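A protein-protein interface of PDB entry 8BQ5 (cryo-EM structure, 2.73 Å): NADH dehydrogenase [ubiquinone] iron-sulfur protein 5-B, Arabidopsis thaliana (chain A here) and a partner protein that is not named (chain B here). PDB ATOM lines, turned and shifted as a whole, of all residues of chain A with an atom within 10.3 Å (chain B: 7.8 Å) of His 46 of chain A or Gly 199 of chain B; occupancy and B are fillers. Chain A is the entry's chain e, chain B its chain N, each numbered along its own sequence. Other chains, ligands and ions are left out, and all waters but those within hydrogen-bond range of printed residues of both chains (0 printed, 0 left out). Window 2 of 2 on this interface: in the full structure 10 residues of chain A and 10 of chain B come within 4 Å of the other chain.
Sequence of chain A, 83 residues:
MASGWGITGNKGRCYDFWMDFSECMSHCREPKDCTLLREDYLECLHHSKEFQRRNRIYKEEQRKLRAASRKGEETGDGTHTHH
Printed residues of chain B within 4 Å of Ala 2 of chain A: Gly 202.
Of the printed residues of chain B, Tyr 41 of chain A touches Thr 201 and Gly 202.
Of the printed residues of chain B, Leu 45 of chain A touches Thr 201 (3.4 Å).
Of chain B, only Gly 199 (3.3 Å) and Ser 200 (3.0 Å) come within 4 Å of His 46 of chain A.
Of chain A, only His 46 comes within 4 Å of Gly 199 of chain B.
Of chain A, only His 46 comes within 4 Å of Ser 200 of chain B.
Of the printed residues of chain A, Thr 201 of chain B touches Tyr 41 and Leu 45.
Printed residues of chain A within 4 Å of Gly 202 of chain B: Ala 2 and Tyr 41.
The nearest printed residue of chain B that does not touch Tyr 41 of chain A is Ala 203 of chain B (4.8 Å).
OG1 of Thr 201 of chain B lies close to N of Ala 203 of chain B, 3.3 Å away.
SG of Cys 44 of chain A is disulfide-bonded to SG of Cys 14 of chain A (2.0 Å).
N of Leu 45 of chain A is in hydrogen-bond range of SG of Cys 14 of chain A (3.6 Å).
NH2 of Arg 13 of chain A sits at hydrogen-bond distance from O of Leu 45 of chain A (3.4 Å).
OG of Ser 200 of chain B is in hydrogen-bond range of OG of Ser 223 of chain B (2.7 Å).
O of Ile 197 of chain B lies within hydrogen-bond range of OG1 of Thr 201 of chain B, at 3.0 Å.
Along chain B the printed residues that touch a printed residue of chain A span positions 199 to 202.
Among the printed residues, no Asp or Glu carboxylate lies within 4 Å of a Lys or Arg side-chain nitrogen of the other chain.
Among the printed residues, pairs that only touch across the chains: His 46 of chain A with Gly 199 of chain B, Leu 45 of chain A with Thr 201 of chain B and Tyr 41 of chain A with Gly 202 of chain B.
The backbone carbonyl oxygen of Ser 200 of chain B sits at hydrogen-bond distance from a ring nitrogen (NE2) of His 46 of chain A.
N of Ala 2 of chain A is in hydrogen-bond range of O of Gly 202 of chain B.
O of Thr 201 of chain B lies within hydrogen-bond range of OH of Tyr 41 of chain A (2.8 Å).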
ATOM      1  N   ALA A   2      21.943  32.670  14.743  1.00  0.00           N
ATOM      2  CA  ALA A   2      23.106  32.735  15.622  1.00  0.00           C
ATOM      3  C   ALA A   2      24.025  33.906  15.279  1.00  0.00           C
ATOM      4  O   ALA A   2      24.826  34.330  16.108  1.00  0.00           O
ATOM      5  CB  ALA A   2      23.882  31.426  15.565  1.00  0.00           C
ATOM      6  N   ARG A  13      15.757  37.462  15.134  1.00  0.00           N
ATOM      7  CA  ARG A  13      14.694  37.111  16.073  1.00  0.00           C
ATOM      8  C   ARG A  13      15.207  36.220  17.196  1.00  0.00           C
ATOM      9  O   ARG A  13      14.841  36.405  18.362  1.00  0.00           O
ATOM     10  CB  ARG A  13      13.546  36.429  15.328  1.00  0.00           C
ATOM     11  CG  ARG A  13      12.589  35.654  16.223  1.00  0.00           C
ATOM     12  CD  ARG A  13      11.463  35.029  15.418  1.00  0.00           C
ATOM     13  NE  ARG A  13      11.713  33.623  15.118  1.00  0.00           N
ATOM     14  CZ  ARG A  13      12.014  33.162  13.912  1.00  0.00           C
ATOM     15  NH1 ARG A  13      12.127  33.972  12.873  1.00  0.00           N
ATOM     16  NH2 ARG A  13      12.210  31.858  13.745  1.00  0.00           N
ATOM     17  N   CYS A  14      16.061  35.255  16.868  1.00  0.00           N
ATOM     18  CA  CYS A  14      16.500  34.240  17.813  1.00  0.00           C
ATOM     19  C   CYS A  14      17.898  34.498  18.357  1.00  0.00           C
ATOM     20  O   CYS A  14      18.497  33.595  18.945  1.00  0.00           O
ATOM     21  CB  CYS A  14      16.441  32.864  17.153  1.00  0.00           C
ATOM     22  SG  CYS A  14      14.789  32.416  16.605  1.00  0.00           S
ATOM     23  N   PHE A  17      18.306  34.377  22.386  1.00  0.00           N
ATOM     24  CA  PHE A  17      18.299  33.000  22.863  1.00  0.00           C
ATOM     25  C   PHE A  17      19.630  32.322  22.573  1.00  0.00           C
ATOM     26  O   PHE A  17      20.183  31.614  23.424  1.00  0.00           O
ATOM     27  CB  PHE A  17      17.156  32.228  22.208  1.00  0.00           C
ATOM     28  CG  PHE A  17      15.807  32.565  22.757  1.00  0.00           C
ATOM     29  CD1 PHE A  17      15.490  32.266  24.067  1.00  0.00           C
ATOM     30  CD2 PHE A  17      14.851  33.173  21.963  1.00  0.00           C
ATOM     31  CE1 PHE A  17      14.250  32.570  24.578  1.00  0.00           C
ATOM     32  CE2 PHE A  17      13.608  33.478  22.470  1.00  0.00           C
ATOM     33  CZ  PHE A  17      13.308  33.178  23.780  1.00  0.00           C
ATOM     34  N   ARG A  38      19.189  25.794  25.395  1.00  0.00           N
ATOM     35  CA  ARG A  38      19.355  25.235  24.059  1.00  0.00           C
ATOM     36  C   ARG A  38      18.010  24.936  23.413  1.00  0.00           C
ATOM     37  O   ARG A  38      17.788  25.254  22.236  1.00  0.00           O
ATOM     38  CB  ARG A  38      20.213  23.973  24.126  1.00  0.00           C
ATOM     39  CG  ARG A  38      20.495  23.337  22.779  1.00  0.00           C
ATOM     40  CD  ARG A  38      20.773  21.858  22.940  1.00  0.00           C
ATOM     41  NE  ARG A  38      21.304  21.244  21.728  1.00  0.00           N
ATOM     42  CZ  ARG A  38      20.637  20.382  20.975  1.00  0.00           C
ATOM     43  NH1 ARG A  38      19.401  20.018  21.270  1.00  0.00           N
ATOM     44  NH2 ARG A  38      21.227  19.869  19.898  1.00  0.00           N
ATOM     45  N   GLU A  39      17.092  24.328  24.168  1.00  0.00           N
ATOM     46  CA  GLU A  39      15.787  24.040  23.592  1.00  0.00           C
ATOM     47  C   GLU A  39      14.961  25.307  23.429  1.00  0.00           C
ATOM     48  O   GLU A  39      14.105  25.368  22.544  1.00  0.00           O
ATOM     49  CB  GLU A  39      15.055  22.975  24.416  1.00  0.00           C
ATOM     50  CG  GLU A  39      14.632  23.362  25.817  1.00  0.00           C
ATOM     51  CD  GLU A  39      14.156  22.157  26.619  1.00  0.00           C
ATOM     52  OE1 GLU A  39      14.897  21.711  27.520  1.00  0.00           O
ATOM     53  OE2 GLU A  39      13.048  21.648  26.342  1.00  0.00           O
ATOM     54  N   ASP A  40      15.236  26.347  24.220  1.00  0.00           N
ATOM     55  CA  ASP A  40      14.612  27.644  23.965  1.00  0.00           C
ATOM     56  C   ASP A  40      15.072  28.227  22.631  1.00  0.00           C
ATOM     57  O   ASP A  40      14.262  28.748  21.852  1.00  0.00           O
ATOM     58  CB  ASP A  40      14.921  28.605  25.110  1.00  0.00           C
ATOM     59  CG  ASP A  40      13.837  28.614  26.164  1.00  0.00           C
ATOM     60  OD1 ASP A  40      13.847  29.519  27.023  1.00  0.00           O
ATOM     61  OD2 ASP A  40      12.973  27.714  26.132  1.00  0.00           O
ATOM     62  N   TYR A  41      16.375  28.152  22.348  1.00  0.00           N
ATOM     63  CA  TYR A  41      16.886  28.647  21.071  1.00  0.00           C
ATOM     64  C   TYR A  41      16.307  27.860  19.898  1.00  0.00           C
ATOM     65  O   TYR A  41      15.889  28.437  18.884  1.00  0.00           O
ATOM     66  CB  TYR A  41      18.414  28.591  21.055  1.00  0.00           C
ATOM     67  CG  TYR A  41      19.018  28.797  19.684  1.00  0.00           C
ATOM     68  CD1 TYR A  41      18.985  30.041  19.067  1.00  0.00           C
ATOM     69  CD2 TYR A  41      19.613  27.745  19.003  1.00  0.00           C
ATOM     70  CE1 TYR A  41      19.534  30.231  17.813  1.00  0.00           C
ATOM     71  CE2 TYR A  41      20.164  27.925  17.752  1.00  0.00           C
ATOM     72  CZ  TYR A  41      20.121  29.170  17.162  1.00  0.00           C
ATOM     73  OH  TYR A  41      20.669  29.348  15.916  1.00  0.00           O
ATOM     74  N   LEU A  42      16.268  26.530  20.020  1.00  0.00           N
ATOM     75  CA  LEU A  42      15.698  25.727  18.941  1.00  0.00           C
ATOM     76  C   LEU A  42      14.198  25.966  18.786  1.00  0.00           C
ATOM     77  O   LEU A  42      13.678  25.940  17.662  1.00  0.00           O
ATOM     78  CB  LEU A  42      15.994  24.244  19.168  1.00  0.00           C
ATOM     79  CG  LEU A  42      17.475  23.867  19.276  1.00  0.00           C
ATOM     80  CD1 LEU A  42      17.646  22.384  19.558  1.00  0.00           C
ATOM     81  CD2 LEU A  42      18.222  24.260  18.012  1.00  0.00           C
ATOM     82  N   GLU A  43      13.489  26.207  19.892  1.00  0.00           N
ATOM     83  CA  GLU A  43      12.072  26.535  19.816  1.00  0.00           C
ATOM     84  C   GLU A  43      11.853  27.866  19.114  1.00  0.00           C
ATOM     85  O   GLU A  43      10.891  28.024  18.354  1.00  0.00           O
ATOM     86  CB  GLU A  43      11.468  26.558  21.222  1.00  0.00           C
ATOM     87  CG  GLU A  43       9.978  26.853  21.270  1.00  0.00           C
ATOM     88  CD  GLU A  43       9.149  25.878  20.458  1.00  0.00           C
ATOM     89  OE1 GLU A  43       9.563  24.711  20.306  1.00  0.00           O
ATOM     90  OE2 GLU A  43       8.074  26.284  19.974  1.00  0.00           O
ATOM     91  N   CYS A  44      12.727  28.841  19.365  1.00  0.00           N
ATOM     92  CA  CYS A  44      12.657  30.082  18.600  1.00  0.00           C
ATOM     93  C   CYS A  44      12.895  29.825  17.120  1.00  0.00           C
ATOM     94  O   CYS A  44      12.228  30.424  16.270  1.00  0.00           O
ATOM     95  CB  CYS A  44      13.670  31.098  19.125  1.00  0.00           C
ATOM     96  SG  CYS A  44      13.634  32.687  18.258  1.00  0.00           S
ATOM     97  N   LEU A  45      13.848  28.948  16.797  1.00  0.00           N
ATOM     98  CA  LEU A  45      14.133  28.662  15.394  1.00  0.00           C
ATOM     99  C   LEU A  45      12.933  28.046  14.686  1.00  0.00           C
ATOM    100  O   LEU A  45      12.538  28.510  13.611  1.00  0.00           O
ATOM    101  CB  LEU A  45      15.338  27.732  15.271  1.00  0.00           C
ATOM    102  CG  LEU A  45      16.721  28.281  15.613  1.00  0.00           C
ATOM    103  CD1 LEU A  45      17.771  27.259  15.223  1.00  0.00           C
ATOM    104  CD2 LEU A  45      16.973  29.608  14.919  1.00  0.00           C
ATOM    105  N   HIS A  46      12.337  27.002  15.265  1.00  0.00           N
ATOM    106  CA  HIS A  46      11.370  26.195  14.533  1.00  0.00           C
ATOM    107  C   HIS A  46       9.943  26.243  15.068  1.00  0.00           C
ATOM    108  O   HIS A  46       9.045  25.724  14.396  1.00  0.00           O
ATOM    109  CB  HIS A  46      11.830  24.730  14.487  1.00  0.00           C
ATOM    110  CG  HIS A  46      13.237  24.557  14.009  1.00  0.00           C
ATOM    111  ND1 HIS A  46      13.649  24.940  12.750  1.00  0.00           N
ATOM    112  CD2 HIS A  46      14.331  24.046  14.622  1.00  0.00           C
ATOM    113  CE1 HIS A  46      14.934  24.670  12.609  1.00  0.00           C
ATOM    114  NE2 HIS A  46      15.371  24.127  13.730  1.00  0.00           N
ATOM    115  N   HIS A  47       9.706  26.835  16.241  1.00  0.00           N
ATOM    116  CA  HIS A  47       8.364  26.936  16.826  1.00  0.00           C
ATOM    117  C   HIS A  47       7.684  25.577  16.960  1.00  0.00           C
ATOM    118  O   HIS A  47       6.462  25.474  16.847  1.00  0.00           O
ATOM    119  CB  HIS A  47       7.465  27.879  16.021  1.00  0.00           C
ATOM    120  CG  HIS A  47       8.096  29.195  15.696  1.00  0.00           C
ATOM    121  ND1 HIS A  47       8.420  30.122  16.660  1.00  0.00           N
ATOM    122  CD2 HIS A  47       8.443  29.747  14.510  1.00  0.00           C
ATOM    123  CE1 HIS A  47       8.949  31.186  16.085  1.00  0.00           C
ATOM    124  NE2 HIS A  47       8.973  30.985  14.780  1.00  0.00           N
ATOM    125  N   SER A  48       8.461  24.525  17.212  1.00  0.00           N
ATOM    126  CA  SER A  48       7.915  23.176  17.124  1.00  0.00           C
ATOM    127  C   SER A  48       6.902  22.905  18.233  1.00  0.00           C
ATOM    128  O   SER A  48       5.814  22.374  17.976  1.00  0.00           O
ATOM    129  CB  SER A  48       9.050  22.153  17.163  1.00  0.00           C
ATOM    130  OG  SER A  48       8.536  20.836  17.125  1.00  0.00           O
ATOM    131  N   LYS A  49       7.232  23.274  19.472  1.00  0.00           N
ATOM    132  CA  LYS A  49       6.345  22.960  20.587  1.00  0.00           C
ATOM    133  C   LYS A  49       5.107  23.849  20.588  1.00  0.00           C
ATOM    134  O   LYS A  49       4.007  23.387  20.916  1.00  0.00           O
ATOM    135  CB  LYS A  49       7.102  23.071  21.908  1.00  0.00           C
ATOM    136  CG  LYS A  49       8.133  21.971  22.094  1.00  0.00           C
ATOM    137  CD  LYS A  49       8.901  22.119  23.394  1.00  0.00           C
ATOM    138  CE  LYS A  49       9.298  23.555  23.653  1.00  0.00           C
ATOM    139  NZ  LYS A  49      10.659  23.837  23.126  1.00  0.00           N
ATOM    140  N   GLU A  50       5.261  25.121  20.222  1.00  0.00           N
ATOM    141  CA  GLU A  50       4.105  26.001  20.095  1.00  0.00           C
ATOM    142  C   GLU A  50       3.110  25.452  19.078  1.00  0.00           C
ATOM    143  O   GLU A  50       1.907  25.343  19.356  1.00  0.00           O
ATOM    144  CB  GLU A  50       4.569  27.402  19.699  1.00  0.00           C
ATOM    145  CG  GLU A  50       3.448  28.387  19.445  1.00  0.00           C
ATOM    146  CD  GLU A  50       3.958  29.761  19.064  1.00  0.00           C
ATOM    147  OE1 GLU A  50       3.127  30.648  18.785  1.00  0.00           O
ATOM    148  OE2 GLU A  50       5.192  29.957  19.050  1.00  0.00           O
ATOM    149  N   PHE A  51       3.603  25.077  17.898  1.00  0.00           N
ATOM    150  CA  PHE A  51       2.724  24.551  16.862  1.00  0.00           C
ATOM    151  C   PHE A  51       2.127  23.212  17.273  1.00  0.00           C
ATOM    152  O   PHE A  51       0.968  22.927  16.962  1.00  0.00           O
ATOM    153  CB  PHE A  51       3.478  24.422  15.539  1.00  0.00           C
ATOM    154  CG  PHE A  51       3.797  25.739  14.892  1.00  0.00           C
ATOM    155  CD1 PHE A  51       3.225  26.913  15.351  1.00  0.00           C
ATOM    156  CD2 PHE A  51       4.671  25.801  13.822  1.00  0.00           C
ATOM    157  CE1 PHE A  51       3.523  28.119  14.755  1.00  0.00           C
ATOM    158  CE2 PHE A  51       4.969  27.004  13.222  1.00  0.00           C
ATOM    159  CZ  PHE A  51       4.396  28.165  13.689  1.00  0.00           C
ATOM    160  N   GLN A  52       2.900  22.377  17.973  1.00  0.00           N
ATOM    161  CA  GLN A  52       2.367  21.098  18.436  1.00  0.00           C
ATOM    162  C   GLN A  52       1.225  21.296  19.425  1.00  0.00           C
ATOM    163  O   GLN A  52       0.198  20.609  19.349  1.00  0.00           O
ATOM    164  CB  GLN A  52       3.477  20.266  19.072  1.00  0.00           C
ATOM    165  CG  GLN A  52       3.052  18.851  19.410  1.00  0.00           C
ATOM    166  CD  GLN A  52       4.183  17.858  19.281  1.00  0.00           C
ATOM    167  OE1 GLN A  52       5.262  18.192  18.799  1.00  0.00           O
ATOM    168  NE2 GLN A  52       3.941  16.626  19.709  1.00  0.00           N
ATOM    169  N   ARG A  54      -0.724  23.988  19.724  1.00  0.00           N
ATOM    170  CA  ARG A  54      -1.876  24.526  19.006  1.00  0.00           C
ATOM    171  C   ARG A  54      -2.563  23.456  18.167  1.00  0.00           C
ATOM    172  O   ARG A  54      -3.792  23.467  18.029  1.00  0.00           O
ATOM    173  CB  ARG A  54      -1.453  25.713  18.144  1.00  0.00           C
ATOM    174  CG  ARG A  54      -1.289  26.997  18.939  1.00  0.00           C
ATOM    175  CD  ARG A  54      -0.312  27.963  18.291  1.00  0.00           C
ATOM    176  NE  ARG A  54      -0.967  28.872  17.358  1.00  0.00           N
ATOM    177  CZ  ARG A  54      -0.396  29.950  16.840  1.00  0.00           C
ATOM    178  NH1 ARG A  54       0.830  30.313  17.178  1.00  0.00           N
ATOM    179  NH2 ARG A  54      -1.072  30.685  15.962  1.00  0.00           N
ATOM    180  N   ASN A  55      -1.797  22.516  17.610  1.00  0.00           N
ATOM    181  CA  ASN A  55      -2.406  21.405  16.892  1.00  0.00           C
ATOM    182  C   ASN A  55      -3.172  20.487  17.833  1.00  0.00           C
ATOM    183  O   ASN A  55      -4.195  19.921  17.440  1.00  0.00           O
ATOM    184  CB  ASN A  55      -1.340  20.626  16.125  1.00  0.00           C
ATOM    185  CG  ASN A  55      -0.798  21.399  14.941  1.00  0.00           C
ATOM    186  OD1 ASN A  55      -1.377  22.401  14.524  1.00  0.00           O
ATOM    187  ND2 ASN A  55       0.318  20.938  14.393  1.00  0.00           N
ATOM    188  N   PHE B 192      24.362  20.729  -0.537  1.00  0.00           N
ATOM    189  CA  PHE B 192      23.090  20.327   0.051  1.00  0.00           C
ATOM    190  C   PHE B 192      23.235  20.004   1.530  1.00  0.00           C
ATOM    191  O   PHE B 192      22.394  20.396   2.351  1.00  0.00           O
ATOM    192  CB  PHE B 192      22.517  19.130  -0.694  1.00  0.00           C
ATOM    193  CG  PHE B 192      21.090  18.897  -0.388  1.00  0.00           C
ATOM    194  CD1 PHE B 192      20.115  19.699  -0.920  1.00  0.00           C
ATOM    195  CD2 PHE B 192      20.729  17.906   0.501  1.00  0.00           C
ATOM    196  CE1 PHE B 192      18.814  19.485  -0.594  1.00  0.00           C
ATOM    197  CE2 PHE B 192      19.419  17.699   0.815  1.00  0.00           C
ATOM    198  CZ  PHE B 192      18.473  18.493   0.263  1.00  0.00           C
ATOM    199  N   GLY B 193      24.279  19.256   1.884  1.00  0.00           N
ATOM    200  CA  GLY B 193      24.520  18.980   3.294  1.00  0.00           C
ATOM    201  C   GLY B 193      24.673  20.247   4.117  1.00  0.00           C
ATOM    202  O   GLY B 193      24.093  20.374   5.203  1.00  0.00           O
ATOM    203  N   CYS B 194      25.449  21.206   3.603  1.00  0.00           N
ATOM    204  CA  CYS B 194      25.629  22.470   4.316  1.00  0.00           C
ATOM    205  C   CYS B 194      24.304  23.202   4.492  1.00  0.00           C
ATOM    206  O   CYS B 194      24.033  23.763   5.561  1.00  0.00           O
ATOM    207  CB  CYS B 194      26.635  23.363   3.587  1.00  0.00           C
ATOM    208  SG  CYS B 194      28.301  22.686   3.434  1.00  0.00           S
ATOM    209  N   SER B 195      23.468  23.214   3.450  1.00  0.00           N
ATOM    210  CA  SER B 195      22.175  23.887   3.550  1.00  0.00           C
ATOM    211  C   SER B 195      21.284  23.221   4.591  1.00  0.00           C
ATOM    212  O   SER B 195      20.588  23.905   5.352  1.00  0.00           O
ATOM    213  CB  SER B 195      21.487  23.917   2.182  1.00  0.00           C
ATOM    214  OG  SER B 195      20.791  22.714   1.918  1.00  0.00           O
ATOM    215  N   MET B 196      21.295  21.888   4.639  1.00  0.00           N
ATOM    216  CA  MET B 196      20.499  21.184   5.639  1.00  0.00           C
ATOM    217  C   MET B 196      20.963  21.529   7.052  1.00  0.00           C
ATOM    218  O   MET B 196      20.141  21.777   7.947  1.00  0.00           O
ATOM    219  CB  MET B 196      20.571  19.674   5.416  1.00  0.00           C
ATOM    220  CG  MET B 196      19.609  19.122   4.370  1.00  0.00           C
ATOM    221  SD  MET B 196      18.095  20.085   4.203  1.00  0.00           S
ATOM    222  CE  MET B 196      17.240  19.671   5.699  1.00  0.00           C
ATOM    223  N   ILE B 197      22.281  21.563   7.264  1.00  0.00           N
ATOM    224  CA  ILE B 197      22.813  21.903   8.583  1.00  0.00           C
ATOM    225  C   ILE B 197      22.413  23.322   8.969  1.00  0.00           C
ATOM    226  O   ILE B 197      21.979  23.581  10.099  1.00  0.00           O
ATOM    227  CB  ILE B 197      24.340  21.726   8.605  1.00  0.00           C
ATOM    228  CG1 ILE B 197      24.696  20.247   8.695  1.00  0.00           C
ATOM    229  CG2 ILE B 197      24.957  22.490   9.768  1.00  0.00           C
ATOM    230  CD1 ILE B 197      26.159  20.005   8.568  1.00  0.00           C
ATOM    231  N   TYR B 198      22.553  24.262   8.033  1.00  0.00           N
ATOM    232  CA  TYR B 198      22.207  25.651   8.314  1.00  0.00           C
ATOM    233  C   TYR B 198      20.733  25.791   8.666  1.00  0.00           C
ATOM    234  O   TYR B 198      20.372  26.501   9.610  1.00  0.00           O
ATOM    235  CB  TYR B 198      22.547  26.530   7.112  1.00  0.00           C
ATOM    236  CG  TYR B 198      22.078  27.955   7.266  1.00  0.00           C
ATOM    237  CD1 TYR B 198      22.581  28.764   8.275  1.00  0.00           C
ATOM    238  CD2 TYR B 198      21.124  28.488   6.412  1.00  0.00           C
ATOM    239  CE1 TYR B 198      22.157  30.064   8.422  1.00  0.00           C
ATOM    240  CE2 TYR B 198      20.693  29.788   6.550  1.00  0.00           C
ATOM    241  CZ  TYR B 198      21.213  30.572   7.557  1.00  0.00           C
ATOM    242  OH  TYR B 198      20.787  31.868   7.700  1.00  0.00           O
ATOM    243  N   GLY B 199      19.863  25.125   7.907  1.00  0.00           N
ATOM    244  CA  GLY B 199      18.445  25.201   8.193  1.00  0.00           C
ATOM    245  C   GLY B 199      18.077  24.597   9.530  1.00  0.00           C
ATOM    246  O   GLY B 199      17.192  25.105  10.223  1.00  0.00           O
ATOM    247  N   SER B 200      18.746  23.510   9.916  1.00  0.00           N
ATOM    248  CA  SER B 200      18.408  22.859  11.176  1.00  0.00           C
ATOM    249  C   SER B 200      18.959  23.601  12.391  1.00  0.00           C
ATOM    250  O   SER B 200      18.313  23.608  13.445  1.00  0.00           O
ATOM    251  CB  SER B 200      18.908  21.416  11.167  1.00  0.00           C
ATOM    252  OG  SER B 200      18.564  20.762  12.373  1.00  0.00           O
ATOM    253  N   THR B 201      20.135  24.225  12.282  1.00  0.00           N
ATOM    254  CA  THR B 201      20.768  24.851  13.438  1.00  0.00           C
ATOM    255  C   THR B 201      20.816  26.372  13.384  1.00  0.00           C
ATOM    256  O   THR B 201      21.085  26.998  14.414  1.00  0.00           O
ATOM    257  CB  THR B 201      22.198  24.322  13.618  1.00  0.00           C
ATOM    258  OG1 THR B 201      23.053  24.896  12.622  1.00  0.00           O
ATOM    259  CG2 THR B 201      22.229  22.808  13.499  1.00  0.00           C
ATOM    260  N   GLY B 202      20.570  26.984  12.228  1.00  0.00           N
ATOM    261  CA  GLY B 202      20.699  28.425  12.131  1.00  0.00           C
ATOM    262  C   GLY B 202      22.114  28.932  12.284  1.00  0.00           C
ATOM    263  O   GLY B 202      22.314  30.078  12.689  1.00  0.00           O
ATOM    264  N   ALA B 203      23.109  28.106  11.969  1.00  0.00           N
ATOM    265  CA  ALA B 203      24.505  28.467  12.156  1.00  0.00           C
ATOM    266  C   ALA B 203      25.355  27.829  11.067  1.00  0.00           C
ATOM    267  O   ALA B 203      25.020  26.766  10.539  1.00  0.00           O
ATOM    268  CB  ALA B 203      25.013  28.030  13.537  1.00  0.00           C
ATOM    269  N   THR B 204      26.464  28.493  10.736  1.00  0.00           N
ATOM    270  CA  THR B 204      27.470  27.927   9.843  1.00  0.00           C
ATOM    271  C   THR B 204      28.887  27.980  10.400  1.00  0.00           C
ATOM    272  O   THR B 204      29.733  27.206   9.940  1.00  0.00           O
ATOM    273  CB  THR B 204      27.450  28.630   8.475  1.00  0.00           C
ATOM    274  OG1 THR B 204      27.356  30.048   8.654  1.00  0.00           O
ATOM    275  CG2 THR B 204      26.268  28.150   7.643  1.00  0.00           C
ATOM    276  N   SER B 223      17.534  15.308  15.404  1.00  0.00           N
ATOM    277  CA  SER B 223      17.305  16.185  14.260  1.00  0.00           C
ATOM    278  C   SER B 223      17.728  15.449  12.998  1.00  0.00           C
ATOM    279  O   SER B 223      18.917  15.245  12.749  1.00  0.00           O
ATOM    280  CB  SER B 223      18.075  17.491  14.421  1.00  0.00           C
ATOM    281  OG  SER B 223      17.817  18.372  13.341  1.00  0.00           O
ATOM    282  N   GLY B 225      17.495  16.555  10.053  1.00  0.00           N
ATOM    283  CA  GLY B 225      18.187  17.500   9.192  1.00  0.00           C
ATOM    284  C   GLY B 225      19.680  17.546   9.456  1.00  0.00           C
ATOM    285  O   GLY B 225      20.486  17.561   8.525  1.00  0.00           O
ATOM    286  N   ILE B 226      20.068  17.565  10.733  1.00  0.00           N
ATOM    287  CA  ILE B 226      21.489  17.559  11.069  1.00  0.00           C
ATOM    288  C   ILE B 226      22.136  16.252  10.628  1.00  0.00           C
ATOM    289  O   ILE B 226      23.250  16.244  10.086  1.00  0.00           O
ATOM    290  CB  ILE B 226      21.688  17.812  12.574  1.00  0.00           C
ATOM    291  CG1 ILE B 226      21.129  19.176  12.963  1.00  0.00           C
ATOM    292  CG2 ILE B 226      23.158  17.767  12.924  1.00  0.00           C
ATOM    293  CD1 ILE B 226      21.166  19.446  14.448  1.00  0.00           C
